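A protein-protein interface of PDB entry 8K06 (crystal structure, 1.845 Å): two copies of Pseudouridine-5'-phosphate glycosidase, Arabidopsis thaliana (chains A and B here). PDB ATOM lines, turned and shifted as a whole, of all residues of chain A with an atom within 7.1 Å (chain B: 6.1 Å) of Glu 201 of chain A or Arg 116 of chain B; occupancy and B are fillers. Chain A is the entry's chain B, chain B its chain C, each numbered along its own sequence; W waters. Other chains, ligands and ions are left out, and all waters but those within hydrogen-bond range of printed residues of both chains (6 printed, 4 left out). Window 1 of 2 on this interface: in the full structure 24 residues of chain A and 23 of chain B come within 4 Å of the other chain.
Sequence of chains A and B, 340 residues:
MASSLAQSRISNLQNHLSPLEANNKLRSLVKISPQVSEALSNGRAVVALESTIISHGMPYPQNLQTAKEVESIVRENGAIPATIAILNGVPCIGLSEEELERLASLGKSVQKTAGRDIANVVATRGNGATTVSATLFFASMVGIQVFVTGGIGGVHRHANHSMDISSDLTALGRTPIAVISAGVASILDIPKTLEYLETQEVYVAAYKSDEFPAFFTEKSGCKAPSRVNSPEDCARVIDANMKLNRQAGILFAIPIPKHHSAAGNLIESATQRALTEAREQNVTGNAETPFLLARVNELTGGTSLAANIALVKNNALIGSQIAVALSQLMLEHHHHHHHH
Water W5 lies within hydrogen-bond range of OE2 of Glu 201 of chain A (2.8 Å), N of Arg 116 of chain B (2.9 Å), OG of Ser 167 of chain B (3.0 Å), N of Gly 115 of chain B (3.1 Å) and OG of Ser 133 of chain B (3.5 Å).
Of chain B, only Gly 115, Arg 116, Ser 133, Ser 167, Thr 170, Ala 171 and Arg 174 come within 4 Å of Glu 201 of chain A.
Arg 116 of chain B touches just these residues of chain A: Glu 198 (3.5 Å), Glu 201 (3.5 Å), Val 202 (2.9 Å), Tyr 203 (3.2 Å), Val 204 (3.8 Å), Pro 225 (3.6 Å) and Arg 246 (3.7 Å).
Of the printed residues of chain B, Gly 173 of chain A touches Arg 174 (2.9 Å).
Printed residues of chain B within 4 Å of Val 204 of chain A: Arg 116 (3.8 Å).
Tyr 196 of chain A touches none of the printed residues of chain B.
Glu 195 of chain A touches none of the printed residues of chain B.
The nearest printed residue of chain B that does not touch Glu 201 of chain A is Ala 114 of chain B (5.4 Å).
The nearest residue of chain A that does not touch Arg 116 of chain B is Leu 197 of chain A (4.4 Å).
The nearest printed residue of chain A that does not touch Ser 167 of chain B is Gln 200 of chain A (5.3 Å).
Of the 15 printed residues of chain B, 9 touch a printed residue of chain A.
Hydrophobic or aromatic side chains of chain B within 4 Å of the printed part of chain A: Ala 119 and Ala 171.
Of the 23 printed residues of chain A, 14 touch a printed residue of chain B.
Hydrophobic or aromatic side chains of chain A within 4 Å of the printed part of chain B: Tyr 203, Val 204, Pro 225 and Val 237.
Among the printed residues, Asp or Glu carboxylates within 4 Å of a Lys or Arg side-chain nitrogen of the other chain: Glu 198 of chain A with Arg 116 of chain B (3.6 Å) and Glu 201 of chain A with Arg 174 of chain B (3.8 Å).
O of Val 202 of chain A lies within hydrogen-bond range of NH1 of Arg 116 of chain B.
The backbone carbonyl oxygen (O) of Gly 173 of chain A sits at hydrogen-bond distance from the guanidinium group (NH1) of Arg 174 of chain B (2.9 Å).
NH2 of Arg 174 of chain B is in salt-bridge range of OE1 of Glu 201 of chain A (3.8 Å).
NE of Arg 246 of chain A is in hydrogen-bond range of O of Gly 115 of chain B (3.4 Å).
The side-chain hydroxyl of Tyr 203 of chain A lies close to the side-chain amide nitrogen of Asn 120 of chain B (3.4 Å).
The guanidinium group (NH2) of Arg 116 of chain B is in salt-bridge range of the side-chain carboxylate (OE1) of Glu 198 of chain A (3.6 Å).
OG1 of Thr 170 of chain B lies within hydrogen-bond range of O of Thr 199 of chain A (2.8 Å).
O of Gln 200 of chain A lies within hydrogen-bond range of NH2 of Arg 174 of chain B.
OD1 of Asn 241 of chain A sits at hydrogen-bond distance from NH1 of Arg 246 of chain A (2.7 Å).
The side-chain hydroxyl (OG) of Ser 133 of chain B sits at hydrogen-bond distance from the side-chain hydroxyl (OG) of Ser 167 of chain B.
No position is printed for both chains.
Among the printed residues, merely in contact across the chains: Tyr 203 of chain A with Arg 116 of chain B (3.2 Å), Glu 201 of chain A with Arg 116 of chain B (3.5 Å), Glu 198 of chain A with Ser 167 of chain B (3.5 Å), Gln 247 of chain A with Arg 174 of chain B (3.5 Å), Pro 225 of chain A with Arg 116 of chain B (3.6 Å), Glu 201 of chain A with Ala 171 of chain B (3.6 Å), Val 237 of chain A with Ala 119 of chain B (3.6 Å), Ser 226 of chain A with Asn 120 of chain B (3.7 Å), Glu 201 of chain A with Gly 115 of chain B (3.7 Å), Thr 199 of chain A with Ser 167 of chain B (3.7 Å), Arg 246 of chain A with Arg 116 of chain B (3.7 Å), Glu 201 of chain A with Ser 133 of chain B (3.8 Å), Glu 201 of chain A with Ser 167 of chain B (3.8 Å), Asn 241 of chain A with Ala 119 of chain B (3.8 Å), Glu 201 of chain A with Thr 170 of chain B (3.8 Å), Val 204 of chain A with Arg 116 of chain B (3.8 Å) and Val 237 of chain A with Asn 120 of chain B (3.9 Å).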
ATOM      1  N   LEU A 172     -31.464 -23.815  28.247  1.00  0.00           N
ATOM      2  CA  LEU A 172     -30.410 -23.664  29.255  1.00  0.00           C
ATOM      3  C   LEU A 172     -29.730 -22.300  29.122  1.00  0.00           C
ATOM      4  O   LEU A 172     -29.342 -21.687  30.115  1.00  0.00           O
ATOM      5  CB  LEU A 172     -29.384 -24.793  29.130  1.00  0.00           C
ATOM      6  CG  LEU A 172     -28.382 -24.936  30.281  1.00  0.00           C
ATOM      7  CD1 LEU A 172     -29.142 -24.880  31.621  1.00  0.00           C
ATOM      8  CD2 LEU A 172     -27.594 -26.242  30.131  1.00  0.00           C
ATOM      9  N   GLY A 173     -29.628 -21.809  27.890  1.00  0.00           N
ATOM     10  CA  GLY A 173     -29.056 -20.494  27.637  1.00  0.00           C
ATOM     11  C   GLY A 173     -29.868 -19.345  28.223  1.00  0.00           C
ATOM     12  O   GLY A 173     -29.372 -18.224  28.366  1.00  0.00           O
ATOM     13  N   LEU A 194     -21.169 -28.338  21.654  1.00  0.00           N
ATOM     14  CA  LEU A 194     -20.341 -27.530  22.550  1.00  0.00           C
ATOM     15  C   LEU A 194     -20.227 -26.085  22.073  1.00  0.00           C
ATOM     16  O   LEU A 194     -20.298 -25.162  22.884  1.00  0.00           O
ATOM     17  CB  LEU A 194     -18.947 -28.146  22.700  1.00  0.00           C
ATOM     18  CG  LEU A 194     -18.861 -29.421  23.529  1.00  0.00           C
ATOM     19  CD1 LEU A 194     -17.425 -29.946  23.491  1.00  0.00           C
ATOM     20  CD2 LEU A 194     -19.322 -29.144  24.956  1.00  0.00           C
ATOM     21  N   GLU A 195     -20.057 -25.886  20.766  1.00  0.00           N
ATOM     22  CA  GLU A 195     -20.005 -24.540  20.192  1.00  0.00           C
ATOM     23  C   GLU A 195     -21.338 -23.799  20.415  1.00  0.00           C
ATOM     24  O   GLU A 195     -21.347 -22.633  20.793  1.00  0.00           O
ATOM     25  CB  GLU A 195     -19.689 -24.583  18.691  1.00  0.00           C
ATOM     26  CG  GLU A 195     -18.301 -25.092  18.324  1.00  0.00           C
ATOM     27  CD  GLU A 195     -17.153 -24.144  18.713  1.00  0.00           C
ATOM     28  OE1 GLU A 195     -17.393 -22.983  19.108  1.00  0.00           O
ATOM     29  OE2 GLU A 195     -15.981 -24.578  18.626  1.00  0.00           O
ATOM     30  N   TYR A 196     -22.453 -24.489  20.201  1.00  0.00           N
ATOM     31  CA  TYR A 196     -23.768 -23.864  20.338  1.00  0.00           C
ATOM     32  C   TYR A 196     -23.987 -23.431  21.792  1.00  0.00           C
ATOM     33  O   TYR A 196     -24.465 -22.337  22.032  1.00  0.00           O
ATOM     34  CB  TYR A 196     -24.864 -24.824  19.886  1.00  0.00           C
ATOM     35  CG  TYR A 196     -26.183 -24.157  19.579  1.00  0.00           C
ATOM     36  CD1 TYR A 196     -27.120 -23.924  20.585  1.00  0.00           C
ATOM     37  CD2 TYR A 196     -26.506 -23.783  18.281  1.00  0.00           C
ATOM     38  CE1 TYR A 196     -28.330 -23.315  20.295  1.00  0.00           C
ATOM     39  CE2 TYR A 196     -27.723 -23.190  17.985  1.00  0.00           C
ATOM     40  CZ  TYR A 196     -28.623 -22.963  19.000  1.00  0.00           C
ATOM     41  OH  TYR A 196     -29.838 -22.386  18.709  1.00  0.00           O
ATOM     42  N   LEU A 197     -23.601 -24.279  22.745  1.00  0.00           N
ATOM     43  CA  LEU A 197     -23.719 -23.929  24.168  1.00  0.00           C
ATOM     44  C   LEU A 197     -22.897 -22.685  24.505  1.00  0.00           C
ATOM     45  O   LEU A 197     -23.357 -21.818  25.232  1.00  0.00           O
ATOM     46  CB  LEU A 197     -23.271 -25.103  25.058  1.00  0.00           C
ATOM     47  CG  LEU A 197     -24.304 -26.252  25.174  1.00  0.00           C
ATOM     48  CD1 LEU A 197     -23.674 -27.529  25.734  1.00  0.00           C
ATOM     49  CD2 LEU A 197     -25.554 -25.849  25.997  1.00  0.00           C
ATOM     50  N   GLU A 198     -21.678 -22.606  23.982  1.00  0.00           N
ATOM     51  CA  GLU A 198     -20.861 -21.407  24.189  1.00  0.00           C
ATOM     52  C   GLU A 198     -21.535 -20.140  23.647  1.00  0.00           C
ATOM     53  O   GLU A 198     -21.563 -19.123  24.328  1.00  0.00           O
ATOM     54  CB  GLU A 198     -19.458 -21.565  23.564  1.00  0.00           C
ATOM     55  CG  GLU A 198     -18.585 -20.325  23.808  1.00  0.00           C
ATOM     56  CD  GLU A 198     -17.139 -20.512  23.389  1.00  0.00           C
ATOM     57  OE1 GLU A 198     -16.802 -21.612  22.909  1.00  0.00           O
ATOM     58  OE2 GLU A 198     -16.332 -19.575  23.599  1.00  0.00           O
ATOM     59  N   THR A 199     -22.094 -20.205  22.442  1.00  0.00           N
ATOM     60  CA  THR A 199     -22.787 -19.060  21.861  1.00  0.00           C
ATOM     61  C   THR A 199     -23.983 -18.638  22.731  1.00  0.00           C
ATOM     62  O   THR A 199     -24.311 -17.451  22.824  1.00  0.00           O
ATOM     63  CB  THR A 199     -23.241 -19.391  20.425  1.00  0.00           C
ATOM     64  OG1 THR A 199     -22.101 -19.857  19.676  1.00  0.00           O
ATOM     65  CG2 THR A 199     -23.859 -18.153  19.722  1.00  0.00           C
ATOM     66  N   GLN A 200     -24.631 -19.609  23.369  1.00  0.00           N
ATOM     67  CA  GLN A 200     -25.794 -19.312  24.218  1.00  0.00           C
ATOM     68  C   GLN A 200     -25.379 -18.839  25.612  1.00  0.00           C
ATOM     69  O   GLN A 200     -26.235 -18.566  26.447  1.00  0.00           O
ATOM     70  CB  GLN A 200     -26.697 -20.554  24.358  1.00  0.00           C
ATOM     71  CG  GLN A 200     -27.345 -20.976  23.041  1.00  0.00           C
ATOM     72  CD  GLN A 200     -28.299 -19.908  22.526  1.00  0.00           C
ATOM     73  OE1 GLN A 200     -29.233 -19.519  23.232  1.00  0.00           O
ATOM     74  NE2 GLN A 200     -28.038 -19.391  21.328  1.00  0.00           N
ATOM     75  N   GLU A 201     -24.078 -18.749  25.842  1.00  0.00           N
ATOM     76  CA  GLU A 201     -23.508 -18.355  27.136  1.00  0.00           C
ATOM     77  C   GLU A 201     -23.792 -19.364  28.266  1.00  0.00           C
ATOM     78  O   GLU A 201     -23.957 -18.978  29.426  1.00  0.00           O
ATOM     79  CB  GLU A 201     -24.007 -16.952  27.553  1.00  0.00           C
ATOM     80  CG  GLU A 201     -23.876 -15.895  26.470  1.00  0.00           C
ATOM     81  CD  GLU A 201     -23.840 -14.493  27.068  1.00  0.00           C
ATOM     82  OE1 GLU A 201     -24.880 -13.809  27.005  1.00  0.00           O
ATOM     83  OE2 GLU A 201     -22.773 -14.094  27.601  1.00  0.00           O
ATOM     84  N   VAL A 202     -23.818 -20.653  27.942  1.00  0.00           N
ATOM     85  CA  VAL A 202     -23.939 -21.661  28.974  1.00  0.00           C
ATOM     86  C   VAL A 202     -22.545 -22.045  29.445  1.00  0.00           C
ATOM     87  O   VAL A 202     -21.705 -22.477  28.655  1.00  0.00           O
ATOM     88  CB  VAL A 202     -24.701 -22.922  28.468  1.00  0.00           C
ATOM     89  CG1 VAL A 202     -24.685 -24.039  29.538  1.00  0.00           C
ATOM     90  CG2 VAL A 202     -26.153 -22.589  28.122  1.00  0.00           C
ATOM     91  N   TYR A 203     -22.287 -21.902  30.740  1.00  0.00           N
ATOM     92  CA  TYR A 203     -21.020 -22.372  31.280  1.00  0.00           C
ATOM     93  C   TYR A 203     -21.007 -23.903  31.261  1.00  0.00           C
ATOM     94  O   TYR A 203     -21.917 -24.540  31.794  1.00  0.00           O
ATOM     95  CB  TYR A 203     -20.814 -21.858  32.708  1.00  0.00           C
ATOM     96  CG  TYR A 203     -19.583 -22.391  33.370  1.00  0.00           C
ATOM     97  CD1 TYR A 203     -18.321 -22.102  32.875  1.00  0.00           C
ATOM     98  CD2 TYR A 203     -19.668 -23.186  34.513  1.00  0.00           C
ATOM     99  CE1 TYR A 203     -17.173 -22.587  33.502  1.00  0.00           C
ATOM    100  CE2 TYR A 203     -18.532 -23.665  35.132  1.00  0.00           C
ATOM    101  CZ  TYR A 203     -17.300 -23.368  34.627  1.00  0.00           C
ATOM    102  OH  TYR A 203     -16.184 -23.878  35.256  1.00  0.00           O
ATOM    103  N   VAL A 204     -19.985 -24.485  30.638  1.00  0.00           N
ATOM    104  CA  VAL A 204     -19.859 -25.951  30.531  1.00  0.00           C
ATOM    105  C   VAL A 204     -18.589 -26.397  31.254  1.00  0.00           C
ATOM    106  O   VAL A 204     -17.500 -25.859  31.004  1.00  0.00           O
ATOM    107  CB  VAL A 204     -19.800 -26.417  29.043  1.00  0.00           C
ATOM    108  CG1 VAL A 204     -19.607 -27.980  28.926  1.00  0.00           C
ATOM    109  CG2 VAL A 204     -21.035 -25.968  28.287  1.00  0.00           C
ATOM    110  N   ALA A 205     -18.712 -27.347  32.173  1.00  0.00           N
ATOM    111  CA  ALA A 205     -17.519 -27.855  32.842  1.00  0.00           C
ATOM    112  C   ALA A 205     -17.590 -29.358  33.000  1.00  0.00           C
ATOM    113  O   ALA A 205     -18.638 -29.909  33.361  1.00  0.00           O
ATOM    114  CB  ALA A 205     -17.342 -27.200  34.198  1.00  0.00           C
ATOM    115  N   PRO A 225     -14.331 -27.440  27.934  1.00  0.00           N
ATOM    116  CA  PRO A 225     -14.017 -26.000  27.933  1.00  0.00           C
ATOM    117  C   PRO A 225     -13.644 -25.480  29.306  1.00  0.00           C
ATOM    118  O   PRO A 225     -12.962 -24.458  29.408  1.00  0.00           O
ATOM    119  CB  PRO A 225     -15.317 -25.340  27.437  1.00  0.00           C
ATOM    120  CG  PRO A 225     -16.361 -26.335  27.653  1.00  0.00           C
ATOM    121  CD  PRO A 225     -15.718 -27.690  27.508  1.00  0.00           C
ATOM    122  N   SER A 226     -14.085 -26.178  30.351  1.00  0.00           N
ATOM    123  CA  SER A 226     -13.707 -25.836  31.719  1.00  0.00           C
ATOM    124  C   SER A 226     -13.762 -27.091  32.590  1.00  0.00           C
ATOM    125  O   SER A 226     -14.292 -28.122  32.183  1.00  0.00           O
ATOM    126  CB  SER A 226     -14.628 -24.756  32.288  1.00  0.00           C
ATOM    127  OG  SER A 226     -14.114 -24.202  33.483  1.00  0.00           O
ATOM    128  N   VAL A 237     -19.766 -22.189  42.018  1.00  0.00           N
ATOM    129  CA  VAL A 237     -20.110 -21.573  40.725  1.00  0.00           C
ATOM    130  C   VAL A 237     -21.608 -21.269  40.645  1.00  0.00           C
ATOM    131  O   VAL A 237     -21.995 -20.185  40.211  1.00  0.00           O
ATOM    132  CB  VAL A 237     -19.702 -22.477  39.533  1.00  0.00           C
ATOM    133  CG1 VAL A 237     -20.112 -21.835  38.200  1.00  0.00           C
ATOM    134  CG2 VAL A 237     -18.210 -22.752  39.566  1.00  0.00           C
ATOM    135  N   ASN A 241     -23.377 -17.581  40.295  1.00  0.00           N
ATOM    136  CA  ASN A 241     -24.317 -17.321  39.216  1.00  0.00           C
ATOM    137  C   ASN A 241     -25.640 -16.777  39.751  1.00  0.00           C
ATOM    138  O   ASN A 241     -26.253 -15.884  39.160  1.00  0.00           O
ATOM    139  CB  ASN A 241     -24.535 -18.600  38.407  1.00  0.00           C
ATOM    140  CG  ASN A 241     -24.985 -18.319  37.002  1.00  0.00           C
ATOM    141  OD1 ASN A 241     -24.338 -17.558  36.280  1.00  0.00           O
ATOM    142  ND2 ASN A 241     -26.082 -18.953  36.584  1.00  0.00           N
ATOM    143  N   ARG A 246     -27.372 -13.783  36.780  1.00  0.00           N
ATOM    144  CA  ARG A 246     -27.256 -14.100  35.361  1.00  0.00           C
ATOM    145  C   ARG A 246     -28.448 -14.951  34.947  1.00  0.00           C
ATOM    146  O   ARG A 246     -28.894 -15.818  35.701  1.00  0.00           O
ATOM    147  CB  ARG A 246     -25.948 -14.832  35.065  1.00  0.00           C
ATOM    148  CG  ARG A 246     -24.776 -13.889  35.002  1.00  0.00           C
ATOM    149  CD  ARG A 246     -23.564 -14.539  34.415  1.00  0.00           C
ATOM    150  NE  ARG A 246     -23.719 -15.006  33.036  1.00  0.00           N
ATOM    151  CZ  ARG A 246     -23.861 -16.304  32.719  1.00  0.00           C
ATOM    152  NH1 ARG A 246     -23.926 -17.223  33.677  1.00  0.00           N
ATOM    153  NH2 ARG A 246     -23.965 -16.688  31.440  1.00  0.00           N
ATOM    154  N   GLN A 247     -28.954 -14.697  33.749  1.00  0.00           N
ATOM    155  CA  GLN A 247     -30.124 -15.395  33.229  1.00  0.00           C
ATOM    156  C   GLN A 247     -29.740 -16.498  32.231  1.00  0.00           C
ATOM    157  O   GLN A 247     -30.435 -16.710  31.241  1.00  0.00           O
ATOM    158  CB  GLN A 247     -31.065 -14.391  32.565  1.00  0.00           C
ATOM    159  CG  GLN A 247     -31.614 -13.369  33.545  1.00  0.00           C
ATOM    160  CD  GLN A 247     -32.314 -14.022  34.728  1.00  0.00           C
ATOM    161  OE1 GLN A 247     -31.955 -13.783  35.881  1.00  0.00           O
ATOM    162  NE2 GLN A 247     -33.310 -14.859  34.447  1.00  0.00           N
ATOM    163  N   ALA A 248     -28.582 -17.111  32.446  1.00  0.00           N
ATOM    164  CA  ALA A 248     -28.124 -18.258  31.670  1.00  0.00           C
ATOM    165  C   ALA A 248     -27.720 -19.367  32.628  1.00  0.00           C
ATOM    166  O   ALA A 248     -27.331 -19.086  33.759  1.00  0.00           O
ATOM    167  CB  ALA A 248     -26.961 -17.885  30.769  1.00  0.00           C
ATOM    168  N   GLY A 249     -27.811 -20.614  32.178  1.00  0.00           N
ATOM    169  CA  GLY A 249     -27.561 -21.744  33.040  1.00  0.00           C
ATOM    170  C   GLY A 249     -26.178 -22.355  32.909  1.00  0.00           C
ATOM    171  O   GLY A 249     -25.260 -21.782  32.293  1.00  0.00           O
ATOM    172  N   ILE A 250     -26.048 -23.525  33.517  1.00  0.00           N
ATOM    173  CA  ILE A 250     -24.782 -24.234  33.652  1.00  0.00           C
ATOM    174  C   ILE A 250     -24.978 -25.691  33.284  1.00  0.00           C
ATOM    175  O   ILE A 250     -26.009 -26.288  33.644  1.00  0.00           O
ATOM    176  CB  ILE A 250     -24.256 -24.132  35.105  1.00  0.00           C
ATOM    177  CG1 ILE A 250     -24.043 -22.670  35.486  1.00  0.00           C
ATOM    178  CG2 ILE A 250     -22.956 -25.008  35.288  1.00  0.00           C
ATOM    179  CD1 ILE A 250     -23.959 -22.442  37.028  1.00  0.00           C
ATOM    180  N   THR B 113     -12.226 -13.870  30.107  1.00  0.00           N
ATOM    181  CA  THR B 113     -13.511 -14.146  30.752  1.00  0.00           C
ATOM    182  C   THR B 113     -14.691 -13.708  29.883  1.00  0.00           C
ATOM    183  O   THR B 113     -14.973 -12.525  29.807  1.00  0.00           O
ATOM    184  CB  THR B 113     -13.582 -13.443  32.130  1.00  0.00           C
ATOM    185  OG1 THR B 113     -12.468 -13.876  32.932  1.00  0.00           O
ATOM    186  CG2 THR B 113     -14.893 -13.805  32.881  1.00  0.00           C
ATOM    187  N   ALA B 114     -15.360 -14.655  29.207  1.00  0.00           N
ATOM    188  CA  ALA B 114     -16.621 -14.328  28.515  1.00  0.00           C
ATOM    189  C   ALA B 114     -17.751 -14.277  29.538  1.00  0.00           C
ATOM    190  O   ALA B 114     -17.534 -14.589  30.712  1.00  0.00           O
ATOM    191  CB  ALA B 114     -16.913 -15.343  27.438  1.00  0.00           C
ATOM    192  N   GLY B 115     -18.953 -13.864  29.133  1.00  0.00           N
ATOM    193  CA  GLY B 115     -20.039 -13.826  30.101  1.00  0.00           C
ATOM    194  C   GLY B 115     -20.259 -15.145  30.837  1.00  0.00           C
ATOM    195  O   GLY B 115     -20.503 -15.166  32.045  1.00  0.00           O
ATOM    196  N   ARG B 116     -20.151 -16.260  30.116  1.00  0.00           N
ATOM    197  CA  ARG B 116     -20.395 -17.576  30.720  1.00  0.00           C
ATOM    198  C   ARG B 116     -19.288 -17.996  31.710  1.00  0.00           C
ATOM    199  O   ARG B 116     -19.464 -18.961  32.445  1.00  0.00           O
ATOM    200  CB  ARG B 116     -20.522 -18.650  29.644  1.00  0.00           C
ATOM    201  CG  ARG B 116     -19.192 -19.011  28.958  1.00  0.00           C
ATOM    202  CD  ARG B 116     -19.428 -20.305  28.213  1.00  0.00           C
ATOM    203  NE  ARG B 116     -18.261 -20.830  27.535  1.00  0.00           N
ATOM    204  CZ  ARG B 116     -18.226 -22.033  26.974  1.00  0.00           C
ATOM    205  NH1 ARG B 116     -19.320 -22.804  26.987  1.00  0.00           N
ATOM    206  NH2 ARG B 116     -17.114 -22.444  26.370  1.00  0.00           N
ATOM    207  N   ASP B 117     -18.173 -17.263  31.739  1.00  0.00           N
ATOM    208  CA  ASP B 117     -17.049 -17.570  32.641  1.00  0.00           C
ATOM    209  C   ASP B 117     -17.073 -16.758  33.927  1.00  0.00           C
ATOM    210  O   ASP B 117     -16.310 -17.042  34.852  1.00  0.00           O
ATOM    211  CB  ASP B 117     -15.702 -17.308  31.958  1.00  0.00           C
ATOM    212  CG  ASP B 117     -15.507 -18.144  30.735  1.00  0.00           C
ATOM    213  OD1 ASP B 117     -15.643 -19.387  30.867  1.00  0.00           O
ATOM    214  OD2 ASP B 117     -15.261 -17.557  29.648  1.00  0.00           O
ATOM    215  N   ILE B 118     -17.924 -15.739  33.981  1.00  0.00           N
ATOM    216  CA  ILE B 118     -17.917 -14.823  35.127  1.00  0.00           C
ATOM    217  C   ILE B 118     -18.106 -15.555  36.443  1.00  0.00           C
ATOM    218  O   ILE B 118     -17.349 -15.332  37.388  1.00  0.00           O
ATOM    219  CB  ILE B 118     -19.012 -13.756  35.011  1.00  0.00           C
ATOM    220  CG1 ILE B 118     -18.733 -12.847  33.806  1.00  0.00           C
ATOM    221  CG2 ILE B 118     -19.094 -12.913  36.320  1.00  0.00           C
ATOM    222  CD1 ILE B 118     -19.887 -11.958  33.454  1.00  0.00           C
ATOM    223  N   ALA B 119     -19.124 -16.416  36.519  1.00  0.00           N
ATOM    224  CA  ALA B 119     -19.426 -17.084  37.775  1.00  0.00           C
ATOM    225  C   ALA B 119     -18.242 -17.924  38.262  1.00  0.00           C
ATOM    226  O   ALA B 119     -17.956 -17.968  39.465  1.00  0.00           O
ATOM    227  CB  ALA B 119     -20.686 -17.964  37.633  1.00  0.00           C
ATOM    228  N   ASN B 120     -17.571 -18.598  37.329  1.00  0.00           N
ATOM    229  CA  ASN B 120     -16.420 -19.419  37.661  1.00  0.00           C
ATOM    230  C   ASN B 120     -15.248 -18.593  38.197  1.00  0.00           C
ATOM    231  O   ASN B 120     -14.604 -18.972  39.165  1.00  0.00           O
ATOM    232  CB  ASN B 120     -15.969 -20.217  36.434  1.00  0.00           C
ATOM    233  CG  ASN B 120     -14.856 -21.218  36.756  1.00  0.00           C
ATOM    234  OD1 ASN B 120     -14.847 -21.836  37.816  1.00  0.00           O
ATOM    235  ND2 ASN B 120     -13.939 -21.397  35.826  1.00  0.00           N
ATOM    236  N   SER B 133     -18.821  -9.854  25.725  1.00  0.00           N
ATOM    237  CA  SER B 133     -20.033 -10.432  26.311  1.00  0.00           C
ATOM    238  C   SER B 133     -20.090 -10.268  27.833  1.00  0.00           C
ATOM    239  O   SER B 133     -21.153 -10.012  28.391  1.00  0.00           O
ATOM    240  CB  SER B 133     -20.191 -11.928  25.948  1.00  0.00           C
ATOM    241  OG  SER B 133     -19.139 -12.728  26.491  1.00  0.00           O
ATOM    242  N   ALA B 134     -18.955 -10.392  28.506  1.00  0.00           N
ATOM    243  CA  ALA B 134     -18.937 -10.230  29.970  1.00  0.00           C
ATOM    244  C   ALA B 134     -19.061  -8.760  30.368  1.00  0.00           C
ATOM    245  O   ALA B 134     -19.735  -8.413  31.353  1.00  0.00           O
ATOM    246  CB  ALA B 134     -17.643 -10.836  30.546  1.00  0.00           C
ATOM    247  N   SER B 167     -20.302 -15.465  21.523  1.00  0.00           N
ATOM    248  CA  SER B 167     -21.406 -15.138  22.423  1.00  0.00           C
ATOM    249  C   SER B 167     -21.615 -13.633  22.484  1.00  0.00           C
ATOM    250  O   SER B 167     -22.634 -13.194  22.987  1.00  0.00           O
ATOM    251  CB  SER B 167     -21.156 -15.686  23.828  1.00  0.00           C
ATOM    252  OG  SER B 167     -20.029 -15.083  24.413  1.00  0.00           O
ATOM    253  N   THR B 170     -25.054 -12.957  20.746  1.00  0.00           N
ATOM    254  CA  THR B 170     -26.253 -13.303  21.495  1.00  0.00           C
ATOM    255  C   THR B 170     -26.392 -12.367  22.696  1.00  0.00           C
ATOM    256  O   THR B 170     -27.496 -11.933  23.024  1.00  0.00           O
ATOM    257  CB  THR B 170     -26.229 -14.766  21.992  1.00  0.00           C
ATOM    258  OG1 THR B 170     -25.337 -14.882  23.085  1.00  0.00           O
ATOM    259  CG2 THR B 170     -25.798 -15.704  20.887  1.00  0.00           C
ATOM    260  N   ALA B 171     -25.266 -12.052  23.340  1.00  0.00           N
ATOM    261  CA  ALA B 171     -25.278 -11.128  24.483  1.00  0.00           C
ATOM    262  C   ALA B 171     -25.856  -9.773  24.081  1.00  0.00           C
ATOM    263  O   ALA B 171     -26.713  -9.220  24.781  1.00  0.00           O
ATOM    264  CB  ALA B 171     -23.857 -10.955  25.067  1.00  0.00           C
ATOM    265  N   ARG B 174     -29.579  -9.586  23.621  1.00  0.00           N
ATOM    266  CA  ARG B 174     -30.472  -9.531  24.765  1.00  0.00           C
ATOM    267  C   ARG B 174     -29.994  -8.611  25.866  1.00  0.00           C
ATOM    268  O   ARG B 174     -30.429  -8.745  27.008  1.00  0.00           O
ATOM    269  CB  ARG B 174     -30.718 -10.926  25.345  1.00  0.00           C
ATOM    270  CG  ARG B 174     -29.491 -11.697  25.738  1.00  0.00           C
ATOM    271  CD  ARG B 174     -29.926 -12.985  26.457  1.00  0.00           C
ATOM    272  NE  ARG B 174     -28.921 -14.032  26.375  1.00  0.00           N
ATOM    273  CZ  ARG B 174     -28.917 -15.145  27.111  1.00  0.00           C
ATOM    274  NH1 ARG B 174     -29.861 -15.368  28.042  1.00  0.00           N
ATOM    275  NH2 ARG B 174     -27.953 -16.035  26.913  1.00  0.00           N
ATOM    276  N   THR B 175     -29.131  -7.665  25.518  1.00  0.00           N
ATOM    277  CA  THR B 175     -28.680  -6.647  26.467  1.00  0.00           C
ATOM    278  C   THR B 175     -28.833  -5.251  25.878  1.00  0.00           C
ATOM    279  O   THR B 175     -28.193  -4.919  24.886  1.00  0.00           O
ATOM    280  CB  THR B 175     -27.210  -6.844  26.856  1.00  0.00           C
ATOM    281  OG1 THR B 175     -26.994  -8.210  27.242  1.00  0.00           O
ATOM    282  CG2 THR B 175     -26.837  -5.901  28.014  1.00  0.00           C
HETATM  283  O   HOH W   1     -17.464 -23.305  29.667  1.00  0.00           O
HETATM  284  O   HOH W   2     -19.683 -17.930  25.770  1.00  0.00           O
HETATM  285  O   HOH W   3     -28.970 -16.798  24.205  1.00  0.00           O
HETATM  286  O   HOH W   4     -23.331 -11.727  28.751  1.00  0.00           O
HETATM  287  O   HOH W   5     -20.528 -15.793  27.266  1.00  0.00           O
HETATM  288  O   HOH W   6     -18.897 -25.223  25.331  1.00  0.00           O
